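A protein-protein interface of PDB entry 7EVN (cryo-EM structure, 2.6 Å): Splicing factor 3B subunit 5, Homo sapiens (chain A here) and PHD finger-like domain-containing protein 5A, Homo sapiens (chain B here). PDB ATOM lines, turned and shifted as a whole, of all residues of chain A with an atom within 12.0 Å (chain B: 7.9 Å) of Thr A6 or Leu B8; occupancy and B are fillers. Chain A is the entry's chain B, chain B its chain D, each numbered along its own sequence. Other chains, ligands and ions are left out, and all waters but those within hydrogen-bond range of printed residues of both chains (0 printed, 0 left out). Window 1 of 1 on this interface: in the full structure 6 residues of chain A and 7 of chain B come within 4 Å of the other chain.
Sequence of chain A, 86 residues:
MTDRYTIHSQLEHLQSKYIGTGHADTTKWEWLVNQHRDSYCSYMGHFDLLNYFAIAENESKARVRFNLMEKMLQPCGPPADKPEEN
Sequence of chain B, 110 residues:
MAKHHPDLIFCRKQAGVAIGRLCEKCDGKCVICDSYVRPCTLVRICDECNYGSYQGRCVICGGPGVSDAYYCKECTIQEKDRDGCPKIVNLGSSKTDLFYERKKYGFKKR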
ATOM      1  N   ARG A   4      28.589  -7.591 -24.110  1.00  0.00           N
ATOM      2  CA  ARG A   4      29.726  -7.182 -24.926  1.00  0.00           C
ATOM      3  C   ARG A   4      29.765  -5.667 -25.118  1.00  0.00           C
ATOM      4  O   ARG A   4      30.736  -5.125 -25.640  1.00  0.00           O
ATOM      5  CB  ARG A   4      29.682  -7.884 -26.286  1.00  0.00           C
ATOM      6  CG  ARG A   4      29.952  -9.373 -26.216  1.00  0.00           C
ATOM      7  CD  ARG A   4      30.140  -9.978 -27.599  1.00  0.00           C
ATOM      8  NE  ARG A   4      31.103  -9.243 -28.413  1.00  0.00           N
ATOM      9  CZ  ARG A   4      32.422  -9.368 -28.307  1.00  0.00           C
ATOM     10  NH1 ARG A   4      32.943 -10.198 -27.414  1.00  0.00           N
ATOM     11  NH2 ARG A   4      33.224  -8.661 -29.092  1.00  0.00           N
ATOM     12  N   TYR A   5      28.697  -4.994 -24.688  1.00  0.00           N
ATOM     13  CA  TYR A   5      28.537  -3.550 -24.832  1.00  0.00           C
ATOM     14  C   TYR A   5      29.274  -2.778 -23.742  1.00  0.00           C
ATOM     15  O   TYR A   5      28.752  -2.611 -22.640  1.00  0.00           O
ATOM     16  CB  TYR A   5      27.060  -3.172 -24.805  1.00  0.00           C
ATOM     17  CG  TYR A   5      26.229  -3.686 -25.953  1.00  0.00           C
ATOM     18  CD1 TYR A   5      24.938  -4.129 -25.737  1.00  0.00           C
ATOM     19  CD2 TYR A   5      26.720  -3.706 -27.248  1.00  0.00           C
ATOM     20  CE1 TYR A   5      24.163  -4.591 -26.767  1.00  0.00           C
ATOM     21  CE2 TYR A   5      25.943  -4.167 -28.294  1.00  0.00           C
ATOM     22  CZ  TYR A   5      24.665  -4.608 -28.042  1.00  0.00           C
ATOM     23  OH  TYR A   5      23.877  -5.077 -29.066  1.00  0.00           O
ATOM     24  N   THR A   6      30.489  -2.317 -24.016  1.00  0.00           N
ATOM     25  CA  THR A   6      31.188  -1.504 -23.034  1.00  0.00           C
ATOM     26  C   THR A   6      31.346  -0.070 -23.525  1.00  0.00           C
ATOM     27  O   THR A   6      31.115   0.242 -24.694  1.00  0.00           O
ATOM     28  CB  THR A   6      32.560  -2.099 -22.715  1.00  0.00           C
ATOM     29  OG1 THR A   6      33.200  -2.516 -23.925  1.00  0.00           O
ATOM     30  CG2 THR A   6      32.413  -3.291 -21.789  1.00  0.00           C
ATOM     31  N   ILE A   7      31.732   0.812 -22.601  1.00  0.00           N
ATOM     32  CA  ILE A   7      32.078   2.183 -22.940  1.00  0.00           C
ATOM     33  C   ILE A   7      33.321   2.257 -23.813  1.00  0.00           C
ATOM     34  O   ILE A   7      33.383   3.087 -24.722  1.00  0.00           O
ATOM     35  CB  ILE A   7      32.253   3.011 -21.644  1.00  0.00           C
ATOM     36  CG1 ILE A   7      30.942   3.685 -21.253  1.00  0.00           C
ATOM     37  CG2 ILE A   7      33.335   4.061 -21.789  1.00  0.00           C
ATOM     38  CD1 ILE A   7      31.015   4.451 -19.962  1.00  0.00           C
ATOM     39  N   HIS A   8      34.301   1.382 -23.578  1.00  0.00           N
ATOM     40  CA  HIS A   8      35.558   1.434 -24.314  1.00  0.00           C
ATOM     41  C   HIS A   8      35.374   1.068 -25.782  1.00  0.00           C
ATOM     42  O   HIS A   8      35.980   1.693 -26.657  1.00  0.00           O
ATOM     43  CB  HIS A   8      36.585   0.511 -23.660  1.00  0.00           C
ATOM     44  CG  HIS A   8      37.702   0.109 -24.570  1.00  0.00           C
ATOM     45  ND1 HIS A   8      38.869   0.832 -24.680  1.00  0.00           N
ATOM     46  CD2 HIS A   8      37.829  -0.941 -25.415  1.00  0.00           C
ATOM     47  CE1 HIS A   8      39.666   0.248 -25.555  1.00  0.00           C
ATOM     48  NE2 HIS A   8      39.058  -0.830 -26.017  1.00  0.00           N
ATOM     49  N   SER A   9      34.565   0.053 -26.077  1.00  0.00           N
ATOM     50  CA  SER A   9      34.304  -0.284 -27.467  1.00  0.00           C
ATOM     51  C   SER A   9      33.331   0.684 -28.122  1.00  0.00           C
ATOM     52  O   SER A   9      33.229   0.698 -29.351  1.00  0.00           O
ATOM     53  CB  SER A   9      33.770  -1.713 -27.587  1.00  0.00           C
ATOM     54  OG  SER A   9      32.953  -2.048 -26.486  1.00  0.00           O
ATOM     55  N   GLN A  10      32.608   1.477 -27.333  1.00  0.00           N
ATOM     56  CA  GLN A  10      31.785   2.532 -27.908  1.00  0.00           C
ATOM     57  C   GLN A  10      32.633   3.740 -28.265  1.00  0.00           C
ATOM     58  O   GLN A  10      32.371   4.421 -29.261  1.00  0.00           O
ATOM     59  CB  GLN A  10      30.673   2.920 -26.936  1.00  0.00           C
ATOM     60  CG  GLN A  10      29.547   3.715 -27.569  1.00  0.00           C
ATOM     61  CD  GLN A  10      28.968   4.753 -26.634  1.00  0.00           C
ATOM     62  OE1 GLN A  10      29.451   4.937 -25.522  1.00  0.00           O
ATOM     63  NE2 GLN A  10      27.940   5.446 -27.086  1.00  0.00           N
ATOM     64  N   LEU A  11      33.661   4.016 -27.463  1.00  0.00           N
ATOM     65  CA  LEU A  11      34.577   5.102 -27.778  1.00  0.00           C
ATOM     66  C   LEU A  11      35.358   4.811 -29.051  1.00  0.00           C
ATOM     67  O   LEU A  11      35.475   5.675 -29.924  1.00  0.00           O
ATOM     68  CB  LEU A  11      35.528   5.334 -26.606  1.00  0.00           C
ATOM     69  CG  LEU A  11      36.779   6.152 -26.899  1.00  0.00           C
ATOM     70  CD1 LEU A  11      36.420   7.598 -27.140  1.00  0.00           C
ATOM     71  CD2 LEU A  11      37.769   6.033 -25.762  1.00  0.00           C
ATOM     72  N   GLU A  12      35.894   3.598 -29.177  1.00  0.00           N
ATOM     73  CA  GLU A  12      36.684   3.253 -30.350  1.00  0.00           C
ATOM     74  C   GLU A  12      35.859   3.241 -31.626  1.00  0.00           C
ATOM     75  O   GLU A  12      36.389   3.574 -32.689  1.00  0.00           O
ATOM     76  CB  GLU A  12      37.350   1.897 -30.147  1.00  0.00           C
ATOM     77  CG  GLU A  12      38.626   1.976 -29.347  1.00  0.00           C
ATOM     78  CD  GLU A  12      39.769   1.226 -29.990  1.00  0.00           C
ATOM     79  OE1 GLU A  12      40.156   1.588 -31.120  1.00  0.00           O
ATOM     80  OE2 GLU A  12      40.289   0.281 -29.362  1.00  0.00           O
ATOM     81  N   HIS A  13      34.584   2.864 -31.551  1.00  0.00           N
ATOM     82  CA  HIS A  13      33.729   2.905 -32.728  1.00  0.00           C
ATOM     83  C   HIS A  13      33.358   4.330 -33.118  1.00  0.00           C
ATOM     84  O   HIS A  13      33.214   4.621 -34.308  1.00  0.00           O
ATOM     85  CB  HIS A  13      32.471   2.073 -32.484  1.00  0.00           C
ATOM     86  CG  HIS A  13      31.406   2.269 -33.517  1.00  0.00           C
ATOM     87  ND1 HIS A  13      30.420   3.222 -33.394  1.00  0.00           N
ATOM     88  CD2 HIS A  13      31.173   1.637 -34.690  1.00  0.00           C
ATOM     89  CE1 HIS A  13      29.626   3.170 -34.447  1.00  0.00           C
ATOM     90  NE2 HIS A  13      30.059   2.214 -35.248  1.00  0.00           N
ATOM     91  N   LEU A  14      33.211   5.231 -32.143  1.00  0.00           N
ATOM     92  CA  LEU A  14      32.943   6.629 -32.459  1.00  0.00           C
ATOM     93  C   LEU A  14      34.180   7.343 -32.982  1.00  0.00           C
ATOM     94  O   LEU A  14      34.054   8.344 -33.691  1.00  0.00           O
ATOM     95  CB  LEU A  14      32.400   7.364 -31.233  1.00  0.00           C
ATOM     96  CG  LEU A  14      30.982   7.041 -30.758  1.00  0.00           C
ATOM     97  CD1 LEU A  14      30.681   7.763 -29.458  1.00  0.00           C
ATOM     98  CD2 LEU A  14      29.945   7.380 -31.816  1.00  0.00           C
ATOM     99  N   GLN A  15      35.374   6.862 -32.637  1.00  0.00           N
ATOM    100  CA  GLN A  15      36.585   7.421 -33.225  1.00  0.00           C
ATOM    101  C   GLN A  15      36.673   7.105 -34.711  1.00  0.00           C
ATOM    102  O   GLN A  15      37.063   7.967 -35.504  1.00  0.00           O
ATOM    103  CB  GLN A  15      37.819   6.894 -32.499  1.00  0.00           C
ATOM    104  CG  GLN A  15      38.054   7.529 -31.141  1.00  0.00           C
ATOM    105  CD  GLN A  15      39.523   7.658 -30.807  1.00  0.00           C
ATOM    106  OE1 GLN A  15      39.912   8.463 -29.966  1.00  0.00           O
ATOM    107  NE2 GLN A  15      40.348   6.856 -31.460  1.00  0.00           N
ATOM    108  N   PRO B   6      30.009  -5.185 -17.752  1.00  0.00           N
ATOM    109  CA  PRO B   6      29.168  -3.990 -17.641  1.00  0.00           C
ATOM    110  C   PRO B   6      28.556  -3.574 -18.975  1.00  0.00           C
ATOM    111  O   PRO B   6      29.292  -3.344 -19.931  1.00  0.00           O
ATOM    112  CB  PRO B   6      30.143  -2.923 -17.131  1.00  0.00           C
ATOM    113  CG  PRO B   6      31.468  -3.365 -17.607  1.00  0.00           C
ATOM    114  CD  PRO B   6      31.439  -4.872 -17.589  1.00  0.00           C
ATOM    115  N   ASP B   7      27.224  -3.502 -19.037  1.00  0.00           N
ATOM    116  CA  ASP B   7      26.516  -3.032 -20.228  1.00  0.00           C
ATOM    117  C   ASP B   7      26.143  -1.563 -20.046  1.00  0.00           C
ATOM    118  O   ASP B   7      24.973  -1.193 -19.966  1.00  0.00           O
ATOM    119  CB  ASP B   7      25.287  -3.894 -20.497  1.00  0.00           C
ATOM    120  CG  ASP B   7      25.623  -5.171 -21.222  1.00  0.00           C
ATOM    121  OD1 ASP B   7      26.824  -5.457 -21.388  1.00  0.00           O
ATOM    122  OD2 ASP B   7      24.691  -5.890 -21.633  1.00  0.00           O
ATOM    123  N   LEU B   8      27.163  -0.715 -19.997  1.00  0.00           N
ATOM    124  CA  LEU B   8      26.983   0.718 -19.820  1.00  0.00           C
ATOM    125  C   LEU B   8      27.738   1.466 -20.906  1.00  0.00           C
ATOM    126  O   LEU B   8      28.939   1.256 -21.091  1.00  0.00           O
ATOM    127  CB  LEU B   8      27.478   1.176 -18.449  1.00  0.00           C
ATOM    128  CG  LEU B   8      26.989   0.429 -17.208  1.00  0.00           C
ATOM    129  CD1 LEU B   8      27.701   0.949 -15.974  1.00  0.00           C
ATOM    130  CD2 LEU B   8      25.487   0.553 -17.044  1.00  0.00           C
ATOM    131  N   ILE B   9      27.035   2.333 -21.626  1.00  0.00           N
ATOM    132  CA  ILE B   9      27.635   3.224 -22.608  1.00  0.00           C
ATOM    133  C   ILE B   9      27.243   4.655 -22.257  1.00  0.00           C
ATOM    134  O   ILE B   9      26.493   4.901 -21.313  1.00  0.00           O
ATOM    135  CB  ILE B   9      27.214   2.877 -24.052  1.00  0.00           C
ATOM    136  CG1 ILE B   9      25.700   2.987 -24.220  1.00  0.00           C
ATOM    137  CG2 ILE B   9      27.684   1.492 -24.425  1.00  0.00           C
ATOM    138  CD1 ILE B   9      25.253   3.001 -25.646  1.00  0.00           C
ATOM    139  N   PHE B  10      27.771   5.603 -23.019  1.00  0.00           N
ATOM    140  CA  PHE B  10      27.329   6.985 -22.942  1.00  0.00           C
ATOM    141  C   PHE B  10      26.241   7.234 -23.978  1.00  0.00           C
ATOM    142  O   PHE B  10      26.131   6.530 -24.980  1.00  0.00           O
ATOM    143  CB  PHE B  10      28.490   7.950 -23.169  1.00  0.00           C
ATOM    144  CG  PHE B  10      29.435   8.057 -22.012  1.00  0.00           C
ATOM    145  CD1 PHE B  10      29.026   8.592 -20.809  1.00  0.00           C
ATOM    146  CD2 PHE B  10      30.747   7.643 -22.135  1.00  0.00           C
ATOM    147  CE1 PHE B  10      29.902   8.699 -19.750  1.00  0.00           C
ATOM    148  CE2 PHE B  10      31.621   7.746 -21.082  1.00  0.00           C
ATOM    149  CZ  PHE B  10      31.198   8.274 -19.886  1.00  0.00           C
ATOM    150  N   CYS B  11      25.422   8.253 -23.722  1.00  0.00           N
ATOM    151  CA  CYS B  11      24.411   8.635 -24.699  1.00  0.00           C
ATOM    152  C   CYS B  11      25.059   9.210 -25.950  1.00  0.00           C
ATOM    153  O   CYS B  11      24.849   8.703 -27.058  1.00  0.00           O
ATOM    154  CB  CYS B  11      23.438   9.639 -24.089  1.00  0.00           C
ATOM    155  SG  CYS B  11      22.216  10.268 -25.255  1.00  0.00           S
ATOM    156  N   ILE B  60      24.790  10.169 -13.480  1.00  0.00           N
ATOM    157  CA  ILE B  60      25.664   9.021 -13.275  1.00  0.00           C
ATOM    158  C   ILE B  60      24.864   7.763 -12.958  1.00  0.00           C
ATOM    159  O   ILE B  60      25.039   6.733 -13.614  1.00  0.00           O
ATOM    160  CB  ILE B  60      26.698   9.311 -12.174  1.00  0.00           C
ATOM    161  CG1 ILE B  60      27.626  10.443 -12.609  1.00  0.00           C
ATOM    162  CG2 ILE B  60      27.513   8.071 -11.875  1.00  0.00           C
ATOM    163  CD1 ILE B  60      28.621  10.854 -11.565  1.00  0.00           C
ATOM    164  N   LYS B  87      25.136  11.299 -20.347  1.00  0.00           N
ATOM    165  CA  LYS B  87      24.303  10.443 -19.518  1.00  0.00           C
ATOM    166  C   LYS B  87      24.682   8.979 -19.711  1.00  0.00           C
ATOM    167  O   LYS B  87      25.003   8.545 -20.819  1.00  0.00           O
ATOM    168  CB  LYS B  87      22.833  10.660 -19.860  1.00  0.00           C
ATOM    169  CG  LYS B  87      21.866  10.067 -18.861  1.00  0.00           C
ATOM    170  CD  LYS B  87      20.863  11.105 -18.406  1.00  0.00           C
ATOM    171  CE  LYS B  87      20.131  10.655 -17.160  1.00  0.00           C
ATOM    172  NZ  LYS B  87      19.368  11.773 -16.544  1.00  0.00           N
ATOM    173  N   ILE B  88      24.647   8.217 -18.626  1.00  0.00           N
ATOM    174  CA  ILE B  88      24.957   6.794 -18.673  1.00  0.00           C
ATOM    175  C   ILE B  88      23.697   6.029 -19.048  1.00  0.00           C
ATOM    176  O   ILE B  88      22.642   6.210 -18.435  1.00  0.00           O
ATOM    177  CB  ILE B  88      25.520   6.304 -17.331  1.00  0.00           C
ATOM    178  CG1 ILE B  88      26.778   7.088 -16.961  1.00  0.00           C
ATOM    179  CG2 ILE B  88      25.818   4.825 -17.397  1.00  0.00           C
ATOM    180  CD1 ILE B  88      28.044   6.549 -17.567  1.00  0.00           C
ATOM    181  N   VAL B  89      23.809   5.175 -20.060  1.00  0.00           N
ATOM    182  CA  VAL B  89      22.694   4.389 -20.568  1.00  0.00           C
ATOM    183  C   VAL B  89      22.903   2.937 -20.176  1.00  0.00           C
ATOM    184  O   VAL B  89      24.005   2.398 -20.321  1.00  0.00           O
ATOM    185  CB  VAL B  89      22.555   4.523 -22.099  1.00  0.00           C
ATOM    186  CG1 VAL B  89      21.253   3.913 -22.565  1.00  0.00           C
ATOM    187  CG2 VAL B  89      22.641   5.974 -22.509  1.00  0.00           C
ATOM    188  N   ASN B  90      21.847   2.304 -19.682  1.00  0.00           N
ATOM    189  CA  ASN B  90      21.878   0.895 -19.312  1.00  0.00           C
ATOM    190  C   ASN B  90      21.318   0.086 -20.475  1.00  0.00           C
ATOM    191  O   ASN B  90      20.113   0.116 -20.740  1.00  0.00           O
ATOM    192  CB  ASN B  90      21.083   0.645 -18.034  1.00  0.00           C
ATOM    193  CG  ASN B  90      21.435  -0.674 -17.378  1.00  0.00           C
ATOM    194  OD1 ASN B  90      21.915  -1.600 -18.028  1.00  0.00           O
ATOM    195  ND2 ASN B  90      21.192  -0.767 -16.079  1.00  0.00           N
ATOM    196  N   LEU B  91      22.197  -0.635 -21.165  1.00  0.00           N
ATOM    197  CA  LEU B  91      21.805  -1.454 -22.301  1.00  0.00           C
ATOM    198  C   LEU B  91      21.275  -2.819 -21.895  1.00  0.00           C
ATOM    199  O   LEU B  91      20.554  -3.442 -22.679  1.00  0.00           O
ATOM    200  CB  LEU B  91      22.991  -1.633 -23.249  1.00  0.00           C
ATOM    201  CG  LEU B  91      23.377  -0.390 -24.046  1.00  0.00           C
ATOM    202  CD1 LEU B  91      24.508  -0.686 -25.001  1.00  0.00           C
ATOM    203  CD2 LEU B  91      22.170   0.141 -24.793  1.00  0.00           C
ATOM    204  N   GLY B  92      21.607  -3.295 -20.700  1.00  0.00           N
ATOM    205  CA  GLY B  92      21.222  -4.628 -20.285  1.00  0.00           C
ATOM    206  C   GLY B  92      19.781  -4.720 -19.839  1.00  0.00           C
ATOM    207  O   GLY B  92      19.230  -5.816 -19.709  1.00  0.00           O
ATOM    208  N   LEU B  98      15.836  -0.736 -14.041  1.00  0.00           N
ATOM    209  CA  LEU B  98      16.879  -0.075 -13.261  1.00  0.00           C
ATOM    210  C   LEU B  98      17.698   0.877 -14.128  1.00  0.00           C
ATOM    211  O   LEU B  98      17.694   0.781 -15.356  1.00  0.00           O
ATOM    212  CB  LEU B  98      17.804  -1.106 -12.609  1.00  0.00           C
ATOM    213  CG  LEU B  98      18.586  -2.028 -13.552  1.00  0.00           C
ATOM    214  CD1 LEU B  98      19.999  -2.252 -13.037  1.00  0.00           C
ATOM    215  CD2 LEU B  98      17.870  -3.353 -13.720  1.00  0.00           C
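OG of Ser A9 is in hydrogen-bond range of OG1 of Thr A6 (2.6 Å).
N of Val B89 lies within hydrogen-bond range of O of Ile B9, 3.0 Å away.
The backbone carbonyl oxygen (O) of Asp B7 is in hydrogen-bond range of the backbone NH (N) of Leu B91 (3.1 Å).
O of Pro B6 sits close to O of Tyr A5.
N of Ile A7 sits close to O of Leu B8, 3.2 Å away.
The side-chain amide nitrogen (NE2) of Gln A10 sits at hydrogen-bond distance from the backbone carbonyl oxygen (O) of Phe B10, at 3.0 Å.
Of chain A, only Tyr A5, Thr A6 and Ile A7 come within 4 Å of Leu B8.
Of chain A, only Arg A4 (3.9 Å) and Tyr A5 (3.3 Å) come within 4 Å of Asp B7.
Phe B10 touches just these residues of chain A: Ile A7 and Gln A10.
No residue of chain A comes within 4 Å of Ile B88.
Of chain A, only Tyr A5 comes within 4 Å of Leu B91.
Of the printed residues of chain B, Gln A10 touches Ile B9 (3.4 Å) and Phe B10 (3.0 Å).
Of the printed residues of chain B, Arg A4 touches Asp B7.
Ile B60 touches none of the printed residues of chain A.
The nearest residue of chain B that does not touch Thr A6 is Asp B7 (5.5 Å).
The nearest printed residue of chain B that does not touch Arg A4 is Pro B6 (5.7 Å).
Among the printed residues, pairs that only touch across the chains: Arg A4 with Asp B7 (3.9 Å), Tyr A5 with Asp B7 (3.3 Å), Tyr A5 with Leu B8 (3.6 Å), Tyr A5 with Leu B91 (3.5 Å), Thr A6 with Pro B6 (3.6 Å), Thr A6 with Leu B8 (3.7 Å), Thr A6 with Ile B9 (3.7 Å), Ile A7 with Ile B9 (3.6 Å), Ile A7 with Phe B10 (3.5 Å) and Gln A10 with Ile B9 (3.4 Å).
Of the 14 printed residues of chain B, 6 touch a printed residue of chain A.
Printed residues of chain B that touch a printed residue of chain A: Pro B6, Asp B7, Leu B8, Ile B9, Phe B10 and Leu B91.
Among the printed residues, 13 pairs touch across the chains.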
